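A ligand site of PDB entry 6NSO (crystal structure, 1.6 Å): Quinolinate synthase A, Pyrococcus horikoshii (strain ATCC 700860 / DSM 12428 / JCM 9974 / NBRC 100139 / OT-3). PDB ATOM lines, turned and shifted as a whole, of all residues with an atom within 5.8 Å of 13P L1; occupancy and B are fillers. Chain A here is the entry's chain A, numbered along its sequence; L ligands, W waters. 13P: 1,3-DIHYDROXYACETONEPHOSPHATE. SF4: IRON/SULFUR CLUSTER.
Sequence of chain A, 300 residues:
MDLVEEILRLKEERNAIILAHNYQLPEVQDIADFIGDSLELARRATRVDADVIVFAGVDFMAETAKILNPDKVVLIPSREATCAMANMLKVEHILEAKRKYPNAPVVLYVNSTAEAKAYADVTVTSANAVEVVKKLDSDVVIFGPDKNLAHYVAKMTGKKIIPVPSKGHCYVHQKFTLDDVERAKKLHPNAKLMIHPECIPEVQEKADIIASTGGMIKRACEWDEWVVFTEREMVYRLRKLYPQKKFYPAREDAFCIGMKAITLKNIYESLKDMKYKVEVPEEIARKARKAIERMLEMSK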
ATOM      1  N   HIS A  21      -9.771   1.675 -22.766  1.00  0.00           N
ATOM      2  CA  HIS A  21     -10.268   0.505 -23.482  1.00  0.00           C
ATOM      3  C   HIS A  21      -9.178  -0.053 -24.393  1.00  0.00           C
ATOM      4  O   HIS A  21      -8.214   0.640 -24.766  1.00  0.00           O
ATOM      5  CB  HIS A  21     -11.508   0.857 -24.323  1.00  0.00           C
ATOM      6  CG  HIS A  21     -12.161  -0.339 -24.951  1.00  0.00           C
ATOM      7  ND1 HIS A  21     -11.870  -0.740 -26.232  1.00  0.00           N
ATOM      8  CD2 HIS A  21     -13.054  -1.238 -24.466  1.00  0.00           C
ATOM      9  CE1 HIS A  21     -12.563  -1.826 -26.529  1.00  0.00           C
ATOM     10  NE2 HIS A  21     -13.285  -2.144 -25.464  1.00  0.00           N
ATOM     11  N   ASN A  22      -9.352  -1.326 -24.764  1.00  0.00           N
ATOM     12  CA  ASN A  22      -8.404  -2.039 -25.623  1.00  0.00           C
ATOM     13  C   ASN A  22      -8.250  -1.414 -27.008  1.00  0.00           C
ATOM     14  O   ASN A  22      -7.246  -1.695 -27.689  1.00  0.00           O
ATOM     15  CB  ASN A  22      -8.862  -3.502 -25.768  1.00  0.00           C
ATOM     16  CG  ASN A  22      -8.600  -4.325 -24.523  1.00  0.00           C
ATOM     17  OD1 ASN A  22      -7.575  -4.159 -23.868  1.00  0.00           O
ATOM     18  ND2 ASN A  22      -9.509  -5.232 -24.214  1.00  0.00           N
ATOM     19  N   TYR A  23      -9.192  -0.595 -27.449  1.00  0.00           N
ATOM     20  CA  TYR A  23      -9.121   0.027 -28.770  1.00  0.00           C
ATOM     21  C   TYR A  23      -8.443   1.393 -28.730  1.00  0.00           C
ATOM     22  O   TYR A  23      -8.417   2.086 -29.752  1.00  0.00           O
ATOM     23  CB  TYR A  23     -10.513   0.199 -29.383  1.00  0.00           C
ATOM     24  CG  TYR A  23     -11.308  -1.085 -29.631  1.00  0.00           C
ATOM     25  CD1 TYR A  23     -10.694  -2.330 -29.666  1.00  0.00           C
ATOM     26  CD2 TYR A  23     -12.699  -1.024 -29.825  1.00  0.00           C
ATOM     27  CE1 TYR A  23     -11.437  -3.484 -29.904  1.00  0.00           C
ATOM     28  CE2 TYR A  23     -13.454  -2.166 -30.061  1.00  0.00           C
ATOM     29  CZ  TYR A  23     -12.814  -3.390 -30.077  1.00  0.00           C
ATOM     30  OH  TYR A  23     -13.555  -4.529 -30.303  1.00  0.00           O
ATOM     31  N   GLY A  36      -8.650  -2.607 -20.531  1.00  0.00           N
ATOM     32  CA  GLY A  36      -9.499  -3.787 -20.564  1.00  0.00           C
ATOM     33  C   GLY A  36     -10.696  -3.616 -21.476  1.00  0.00           C
ATOM     34  O   GLY A  36     -10.857  -2.576 -22.129  1.00  0.00           O
ATOM     35  N   ASP A  37     -11.532  -4.655 -21.508  1.00  0.00           N
ATOM     36  CA  ASP A  37     -12.763  -4.618 -22.283  1.00  0.00           C
ATOM     37  C   ASP A  37     -13.875  -3.973 -21.458  1.00  0.00           C
ATOM     38  O   ASP A  37     -13.647  -3.414 -20.385  1.00  0.00           O
ATOM     39  CB  ASP A  37     -13.139  -6.015 -22.804  1.00  0.00           C
ATOM     40  CG  ASP A  37     -13.666  -6.991 -21.727  1.00  0.00           C
ATOM     41  OD1 ASP A  37     -13.756  -6.662 -20.531  1.00  0.00           O
ATOM     42  OD2 ASP A  37     -14.018  -8.132 -22.136  1.00  0.00           O
ATOM     43  N   SER A  38     -15.100  -4.014 -21.995  1.00  0.00           N
ATOM     44  CA  SER A  38     -16.216  -3.346 -21.325  1.00  0.00           C
ATOM     45  C   SER A  38     -16.467  -3.943 -19.944  1.00  0.00           C
ATOM     46  O   SER A  38     -16.712  -3.208 -18.982  1.00  0.00           O
ATOM     47  CB  SER A  38     -17.480  -3.429 -22.187  1.00  0.00           C
ATOM     48  OG  SER A  38     -17.300  -2.779 -23.446  1.00  0.00           O
ATOM     49  N   LEU A  39     -16.418  -5.280 -19.845  1.00  0.00           N
ATOM     50  CA  LEU A  39     -16.749  -5.957 -18.591  1.00  0.00           C
ATOM     51  C   LEU A  39     -15.667  -5.737 -17.537  1.00  0.00           C
ATOM     52  O   LEU A  39     -15.977  -5.540 -16.353  1.00  0.00           O
ATOM     53  CB  LEU A  39     -16.944  -7.457 -18.842  1.00  0.00           C
ATOM     54  CG  LEU A  39     -17.352  -8.276 -17.609  1.00  0.00           C
ATOM     55  CD1 LEU A  39     -18.532  -7.636 -16.895  1.00  0.00           C
ATOM     56  CD2 LEU A  39     -17.681  -9.723 -17.967  1.00  0.00           C
ATOM     57  N   VAL A  58     -15.148   5.503 -24.907  1.00  0.00           N
ATOM     58  CA  VAL A  58     -16.276   6.253 -25.459  1.00  0.00           C
ATOM     59  C   VAL A  58     -17.298   6.506 -24.361  1.00  0.00           C
ATOM     60  O   VAL A  58     -17.210   5.944 -23.263  1.00  0.00           O
ATOM     61  CB  VAL A  58     -16.935   5.567 -26.675  1.00  0.00           C
ATOM     62  CG1 VAL A  58     -15.970   5.546 -27.840  1.00  0.00           C
ATOM     63  CG2 VAL A  58     -17.412   4.167 -26.307  1.00  0.00           C
ATOM     64  N   PHE A  60     -20.499   5.851 -23.472  1.00  0.00           N
ATOM     65  CA  PHE A  60     -21.292   4.928 -22.656  1.00  0.00           C
ATOM     66  C   PHE A  60     -20.423   4.234 -21.612  1.00  0.00           C
ATOM     67  O   PHE A  60     -20.919   3.839 -20.550  1.00  0.00           O
ATOM     68  CB  PHE A  60     -22.034   3.899 -23.538  1.00  0.00           C
ATOM     69  CG  PHE A  60     -21.143   2.817 -24.145  1.00  0.00           C
ATOM     70  CD1 PHE A  60     -20.722   1.719 -23.380  1.00  0.00           C
ATOM     71  CD2 PHE A  60     -20.794   2.857 -25.480  1.00  0.00           C
ATOM     72  CE1 PHE A  60     -19.923   0.740 -23.941  1.00  0.00           C
ATOM     73  CE2 PHE A  60     -19.993   1.857 -26.047  1.00  0.00           C
ATOM     74  CZ  PHE A  60     -19.559   0.806 -25.278  1.00  0.00           C
ATOM     75  N   MET A  61     -19.110   4.118 -21.893  1.00  0.00           N
ATOM     76  CA  MET A  61     -18.186   3.484 -20.978  1.00  0.00           C
ATOM     77  C   MET A  61     -17.867   4.387 -19.799  1.00  0.00           C
ATOM     78  O   MET A  61     -17.870   3.935 -18.649  1.00  0.00           O
ATOM     79  CB  MET A  61     -16.905   3.120 -21.728  1.00  0.00           C
ATOM     80  CG  MET A  61     -17.118   2.113 -22.843  1.00  0.00           C
ATOM     81  SD  MET A  61     -15.516   1.659 -23.563  1.00  0.00           S
ATOM     82  CE  MET A  61     -16.044   0.367 -24.680  1.00  0.00           C
ATOM     83  N   MET A  85     -23.236   2.564 -32.438  1.00  0.00           N
ATOM     84  CA  MET A  85     -24.205   1.494 -32.223  1.00  0.00           C
ATOM     85  C   MET A  85     -25.025   1.734 -30.966  1.00  0.00           C
ATOM     86  O   MET A  85     -26.233   1.489 -30.942  1.00  0.00           O
ATOM     87  CB  MET A  85     -23.465   0.151 -32.143  1.00  0.00           C
ATOM     88  CG  MET A  85     -24.350  -1.046 -31.769  1.00  0.00           C
ATOM     89  SD  MET A  85     -24.112  -1.679 -30.087  1.00  0.00           S
ATOM     90  CE  MET A  85     -22.502  -2.450 -30.297  1.00  0.00           C
ATOM     91  N   TYR A 109     -27.067  -4.704 -23.856  1.00  0.00           N
ATOM     92  CA  TYR A 109     -25.636  -4.564 -24.038  1.00  0.00           C
ATOM     93  C   TYR A 109     -25.174  -3.273 -23.369  1.00  0.00           C
ATOM     94  O   TYR A 109     -25.852  -2.235 -23.437  1.00  0.00           O
ATOM     95  CB  TYR A 109     -25.361  -4.518 -25.544  1.00  0.00           C
ATOM     96  CG  TYR A 109     -23.997  -4.919 -26.039  1.00  0.00           C
ATOM     97  CD1 TYR A 109     -23.087  -5.604 -25.235  1.00  0.00           C
ATOM     98  CD2 TYR A 109     -23.633  -4.635 -27.342  1.00  0.00           C
ATOM     99  CE1 TYR A 109     -21.839  -5.960 -25.720  1.00  0.00           C
ATOM    100  CE2 TYR A 109     -22.412  -4.975 -27.826  1.00  0.00           C
ATOM    101  CZ  TYR A 109     -21.509  -5.640 -27.029  1.00  0.00           C
ATOM    102  OH  TYR A 109     -20.297  -5.969 -27.557  1.00  0.00           O
ATOM    103  N   ASN A 111     -23.134  -1.369 -24.414  1.00  0.00           N
ATOM    104  CA  ASN A 111     -23.131  -0.347 -25.451  1.00  0.00           C
ATOM    105  C   ASN A 111     -24.541   0.242 -25.573  1.00  0.00           C
ATOM    106  O   ASN A 111     -25.281  -0.026 -26.526  1.00  0.00           O
ATOM    107  CB  ASN A 111     -22.647  -0.922 -26.787  1.00  0.00           C
ATOM    108  CG  ASN A 111     -21.274  -1.557 -26.699  1.00  0.00           C
ATOM    109  OD1 ASN A 111     -20.979  -2.294 -25.752  1.00  0.00           O
ATOM    110  ND2 ASN A 111     -20.422  -1.272 -27.681  1.00  0.00           N
ATOM    111  N   THR A 125     -22.244  -7.657 -21.413  1.00  0.00           N
ATOM    112  CA  THR A 125     -21.225  -7.326 -22.397  1.00  0.00           C
ATOM    113  C   THR A 125     -21.050  -8.533 -23.297  1.00  0.00           C
ATOM    114  O   THR A 125     -21.631  -9.592 -23.076  1.00  0.00           O
ATOM    115  CB  THR A 125     -19.901  -6.945 -21.734  1.00  0.00           C
ATOM    116  OG1 THR A 125     -19.168  -8.145 -21.462  1.00  0.00           O
ATOM    117  CG2 THR A 125     -20.161  -6.223 -20.420  1.00  0.00           C
ATOM    118  N   SER A 126     -20.211  -8.376 -24.327  1.00  0.00           N
ATOM    119  CA  SER A 126     -19.908  -9.481 -25.213  1.00  0.00           C
ATOM    120  C   SER A 126     -19.353 -10.679 -24.442  1.00  0.00           C
ATOM    121  O   SER A 126     -19.562 -11.829 -24.831  1.00  0.00           O
ATOM    122  CB  SER A 126     -18.914  -9.042 -26.277  1.00  0.00           C
ATOM    123  OG  SER A 126     -17.935  -8.171 -25.730  1.00  0.00           O
ATOM    124  N   ALA A 127     -18.662 -10.424 -23.323  1.00  0.00           N
ATOM    125  CA  ALA A 127     -18.026 -11.510 -22.591  1.00  0.00           C
ATOM    126  C   ALA A 127     -19.030 -12.367 -21.822  1.00  0.00           C
ATOM    127  O   ALA A 127     -18.790 -13.569 -21.646  1.00  0.00           O
ATOM    128  CB  ALA A 127     -16.978 -10.944 -21.620  1.00  0.00           C
ATOM    129  N   CYS A 170     -22.503  -2.483 -35.317  1.00  0.00           N
ATOM    130  CA  CYS A 170     -21.282  -1.709 -35.243  1.00  0.00           C
ATOM    131  C   CYS A 170     -20.654  -1.642 -36.638  1.00  0.00           C
ATOM    132  O   CYS A 170     -20.316  -2.692 -37.200  1.00  0.00           O
ATOM    133  CB  CYS A 170     -20.318  -2.338 -34.230  1.00  0.00           C
ATOM    134  SG  CYS A 170     -18.652  -1.746 -34.461  1.00  0.00           S
ATOM    135  N   HIS A 173     -17.175  -3.513 -36.981  1.00  0.00           N
ATOM    136  CA  HIS A 173     -17.182  -4.972 -37.105  1.00  0.00           C
ATOM    137  C   HIS A 173     -17.962  -5.460 -38.321  1.00  0.00           C
ATOM    138  O   HIS A 173     -17.675  -6.543 -38.836  1.00  0.00           O
ATOM    139  CB  HIS A 173     -17.710  -5.570 -35.806  1.00  0.00           C
ATOM    140  CG  HIS A 173     -16.720  -5.435 -34.698  1.00  0.00           C
ATOM    141  ND1 HIS A 173     -16.764  -4.400 -33.784  1.00  0.00           N
ATOM    142  CD2 HIS A 173     -15.627  -6.172 -34.380  1.00  0.00           C
ATOM    143  CE1 HIS A 173     -15.759  -4.531 -32.939  1.00  0.00           C
ATOM    144  NE2 HIS A 173     -15.044  -5.581 -33.290  1.00  0.00           N
ATOM    145  N   HIS A 196     -14.682 -11.195 -33.162  1.00  0.00           N
ATOM    146  CA  HIS A 196     -15.589 -10.564 -32.225  1.00  0.00           C
ATOM    147  C   HIS A 196     -17.034 -10.921 -32.584  1.00  0.00           C
ATOM    148  O   HIS A 196     -17.377 -10.980 -33.772  1.00  0.00           O
ATOM    149  CB  HIS A 196     -15.389  -9.044 -32.269  1.00  0.00           C
ATOM    150  CG  HIS A 196     -15.901  -8.334 -31.061  1.00  0.00           C
ATOM    151  ND1 HIS A 196     -17.238  -8.045 -30.876  1.00  0.00           N
ATOM    152  CD2 HIS A 196     -15.260  -7.895 -29.937  1.00  0.00           C
ATOM    153  CE1 HIS A 196     -17.393  -7.435 -29.713  1.00  0.00           C
ATOM    154  NE2 HIS A 196     -16.220  -7.346 -29.115  1.00  0.00           N
ATOM    155  N   GLU A 198     -19.554  -9.089 -32.559  1.00  0.00           N
ATOM    156  CA  GLU A 198     -20.206  -8.023 -33.314  1.00  0.00           C
ATOM    157  C   GLU A 198     -20.008  -8.176 -34.818  1.00  0.00           C
ATOM    158  O   GLU A 198     -20.628  -7.429 -35.584  1.00  0.00           O
ATOM    159  CB  GLU A 198     -19.700  -6.648 -32.864  1.00  0.00           C
ATOM    160  CG  GLU A 198     -20.255  -6.220 -31.512  1.00  0.00           C
ATOM    161  CD  GLU A 198     -19.586  -4.978 -30.927  1.00  0.00           C
ATOM    162  OE1 GLU A 198     -18.984  -4.192 -31.689  1.00  0.00           O
ATOM    163  OE2 GLU A 198     -19.673  -4.785 -29.692  1.00  0.00           O
ATOM    164  N   ALA A 211     -15.074 -14.248 -29.328  1.00  0.00           N
ATOM    165  CA  ALA A 211     -14.801 -13.750 -27.997  1.00  0.00           C
ATOM    166  C   ALA A 211     -14.866 -12.233 -28.013  1.00  0.00           C
ATOM    167  O   ALA A 211     -14.631 -11.607 -29.047  1.00  0.00           O
ATOM    168  CB  ALA A 211     -13.435 -14.237 -27.504  1.00  0.00           C
ATOM    169  N   SER A 212     -15.213 -11.661 -26.853  1.00  0.00           N
ATOM    170  CA  SER A 212     -14.971 -10.265 -26.547  1.00  0.00           C
ATOM    171  C   SER A 212     -13.471 -10.011 -26.610  1.00  0.00           C
ATOM    172  O   SER A 212     -12.670 -10.943 -26.642  1.00  0.00           O
ATOM    173  CB  SER A 212     -15.498  -9.930 -25.149  1.00  0.00           C
ATOM    174  OG  SER A 212     -14.669 -10.512 -24.142  1.00  0.00           O
ATOM    175  N   THR A 213     -13.068  -8.732 -26.612  1.00  0.00           N
ATOM    176  CA  THR A 213     -11.637  -8.455 -26.567  1.00  0.00           C
ATOM    177  C   THR A 213     -11.004  -9.023 -25.308  1.00  0.00           C
ATOM    178  O   THR A 213      -9.865  -9.507 -25.353  1.00  0.00           O
ATOM    179  CB  THR A 213     -11.348  -6.959 -26.674  1.00  0.00           C
ATOM    180  OG1 THR A 213     -11.814  -6.276 -25.503  1.00  0.00           O
ATOM    181  CG2 THR A 213     -12.008  -6.403 -27.898  1.00  0.00           C
ATOM    182  N   GLY A 214     -11.729  -9.012 -24.183  1.00  0.00           N
ATOM    183  CA  GLY A 214     -11.216  -9.639 -22.977  1.00  0.00           C
ATOM    184  C   GLY A 214     -10.986 -11.131 -23.159  1.00  0.00           C
ATOM    185  O   GLY A 214      -9.964 -11.671 -22.722  1.00  0.00           O
ATOM    186  N   THR A 230     -11.203  -7.733 -35.103  1.00  0.00           N
ATOM    187  CA  THR A 230     -11.863  -6.643 -34.365  1.00  0.00           C
ATOM    188  C   THR A 230     -11.120  -5.340 -34.703  1.00  0.00           C
ATOM    189  O   THR A 230     -10.297  -5.299 -35.621  1.00  0.00           O
ATOM    190  CB  THR A 230     -11.925  -6.952 -32.857  1.00  0.00           C
ATOM    191  OG1 THR A 230     -12.743  -5.989 -32.164  1.00  0.00           O
ATOM    192  CG2 THR A 230     -10.533  -6.979 -32.247  1.00  0.00           C
ATOM    193  N   MET A 259     -13.506   5.949 -30.588  1.00  0.00           N
ATOM    194  CA  MET A 259     -12.375   5.593 -29.742  1.00  0.00           C
ATOM    195  C   MET A 259     -11.202   6.543 -29.984  1.00  0.00           C
ATOM    196  O   MET A 259     -10.556   7.000 -29.025  1.00  0.00           O
ATOM    197  CB  MET A 259     -11.955   4.150 -30.028  1.00  0.00           C
ATOM    198  CG  MET A 259     -12.873   3.112 -29.386  1.00  0.00           C
ATOM    199  SD  MET A 259     -12.761   3.144 -27.576  1.00  0.00           S
ATOM    200  CE  MET A 259     -13.939   1.885 -27.194  1.00  0.00           C
HETATM  201  P   13P L   1     -15.362  -5.674 -25.726  1.00  0.00           P
HETATM  202  O1P 13P L   1     -15.224  -6.870 -26.682  1.00  0.00           O
HETATM  203  O2P 13P L   1     -16.188  -5.828 -24.480  1.00  0.00           O
HETATM  204  O3P 13P L   1     -14.163  -4.776 -25.720  1.00  0.00           O
HETATM  205  O1  13P L   1     -16.437  -4.666 -26.804  1.00  0.00           O
HETATM  206  C1  13P L   1     -15.666  -3.953 -27.677  1.00  0.00           C
HETATM  207  C2  13P L   1     -16.606  -3.176 -28.558  1.00  0.00           C
HETATM  208  O2  13P L   1     -16.862  -3.417 -29.713  1.00  0.00           O
HETATM  209  C3  13P L   1     -17.251  -1.977 -27.909  1.00  0.00           C
HETATM  210  O3  13P L   1     -16.336  -0.983 -28.055  1.00  0.00           O
HETATM  211 FE1  SF4 L   2     -17.261  -0.457 -30.134  1.00  0.00          FE
HETATM  212 FE2  SF4 L   2     -19.164   1.339 -30.716  1.00  0.00          FE
HETATM  213 FE3  SF4 L   2     -18.205  -0.218 -32.622  1.00  0.00          FE
HETATM  214 FE4  SF4 L   2     -16.674   1.782 -31.696  1.00  0.00          FE
HETATM  215  S1  SF4 L   2     -18.621   1.968 -32.781  1.00  0.00           S
HETATM  216  S2  SF4 L   2     -16.077  -0.304 -32.003  1.00  0.00           S
HETATM  217  S3  SF4 L   2     -17.320   1.652 -29.590  1.00  0.00           S
HETATM  218  S4  SF4 L   2     -19.307  -0.856 -30.840  1.00  0.00           S
HETATM  219  O   HOH W   1     -16.609  -7.227 -22.161  1.00  0.00           O
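Water W1 lies within hydrogen-bond range of an oxygen (O2P) of 13P L1, the side-chain carboxylate (OD2) of Asp 37, the side-chain hydroxyl (OG1) of Thr 125 and the backbone NH (N) of Leu 39.
The side-chain carboxylate (OE1) of Glu 198 lies close to an oxygen (O2) of 13P L1, 3.0 Å away.
Merely in contact with 13P L1: Tyr 23 (3.4 Å), Asp 37 (3.3 Å), Met 61 (3.6 Å), Asn 111 (3.3 Å), His 173 (3.6 Å), Ser 212 (3.4 Å) and Met 259 (3.8 Å).
Hydrophobic or aromatic side chains within 4 Å of 13P L1: His 21, Tyr 23, Met 61, His 173, His 196 and Met 259.
O3 of 13P L1 is bound to FE1 of SF4 L2 (2.3 Å).
The side-chain hydroxyl of Thr 213 sits at hydrogen-bond distance from the side-chain amide nitrogen of Asn 22 (2.8 Å).
The side-chain carboxylate (OE1) of Glu 198 lies close to the side-chain sulfur (SG) of Cys 170 (3.7 Å).
OD2 of Asp 37 sits at hydrogen-bond distance from OG of Ser 212, 3.2 Å away.
The backbone NH (N) of Leu 39 lies within hydrogen-bond range of the side-chain carboxylate (OD1) of Asp 37 (3.1 Å).
OD2 of Asp 37 lies within hydrogen-bond range of N of Gly 214.
The side-chain hydroxyl of Tyr 23 sits close to a ring nitrogen (NE2) of His 173 (3.5 Å).
OH of Tyr 23 sits at hydrogen-bond distance from OG1 of Thr 230 (2.5 Å).
The side-chain hydroxyl (OG1) of Thr 230 is in hydrogen-bond range of a ring nitrogen (NE2) of His 173 (2.6 Å).
A ring nitrogen (NE2) of His 196 sits at hydrogen-bond distance from an oxygen (O1P) of 13P L1 (2.7 Å).
An oxygen (O3P) of 13P L1 lies within hydrogen-bond range of a ring nitrogen (NE2) of His 21 (2.8 Å).
The backbone NH (N) of Thr 213 lies within hydrogen-bond range of an oxygen (O1P) of 13P L1, at 2.8 Å.
The side-chain hydroxyl of Thr 213 is in hydrogen-bond range of an oxygen (O3P) of 13P L1.
The side-chain hydroxyl (OG) of Ser 126 lies within hydrogen-bond range of an oxygen (O1P) of 13P L1 (3.2 Å).
O2P of 13P L1 sits at hydrogen-bond distance from N of Ser 38.
OG of Ser 38 lies within hydrogen-bond range of O2P of 13P L1.
A sulfur (S4) of SF4 L2 sits close to the side-chain amide nitrogen (ND2) of Asn 111, 3.4 Å away.
An iron atom (FE3) of SF4 L2 is bound by the side-chain sulfur (SG) of Cys 170 (2.4 Å).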
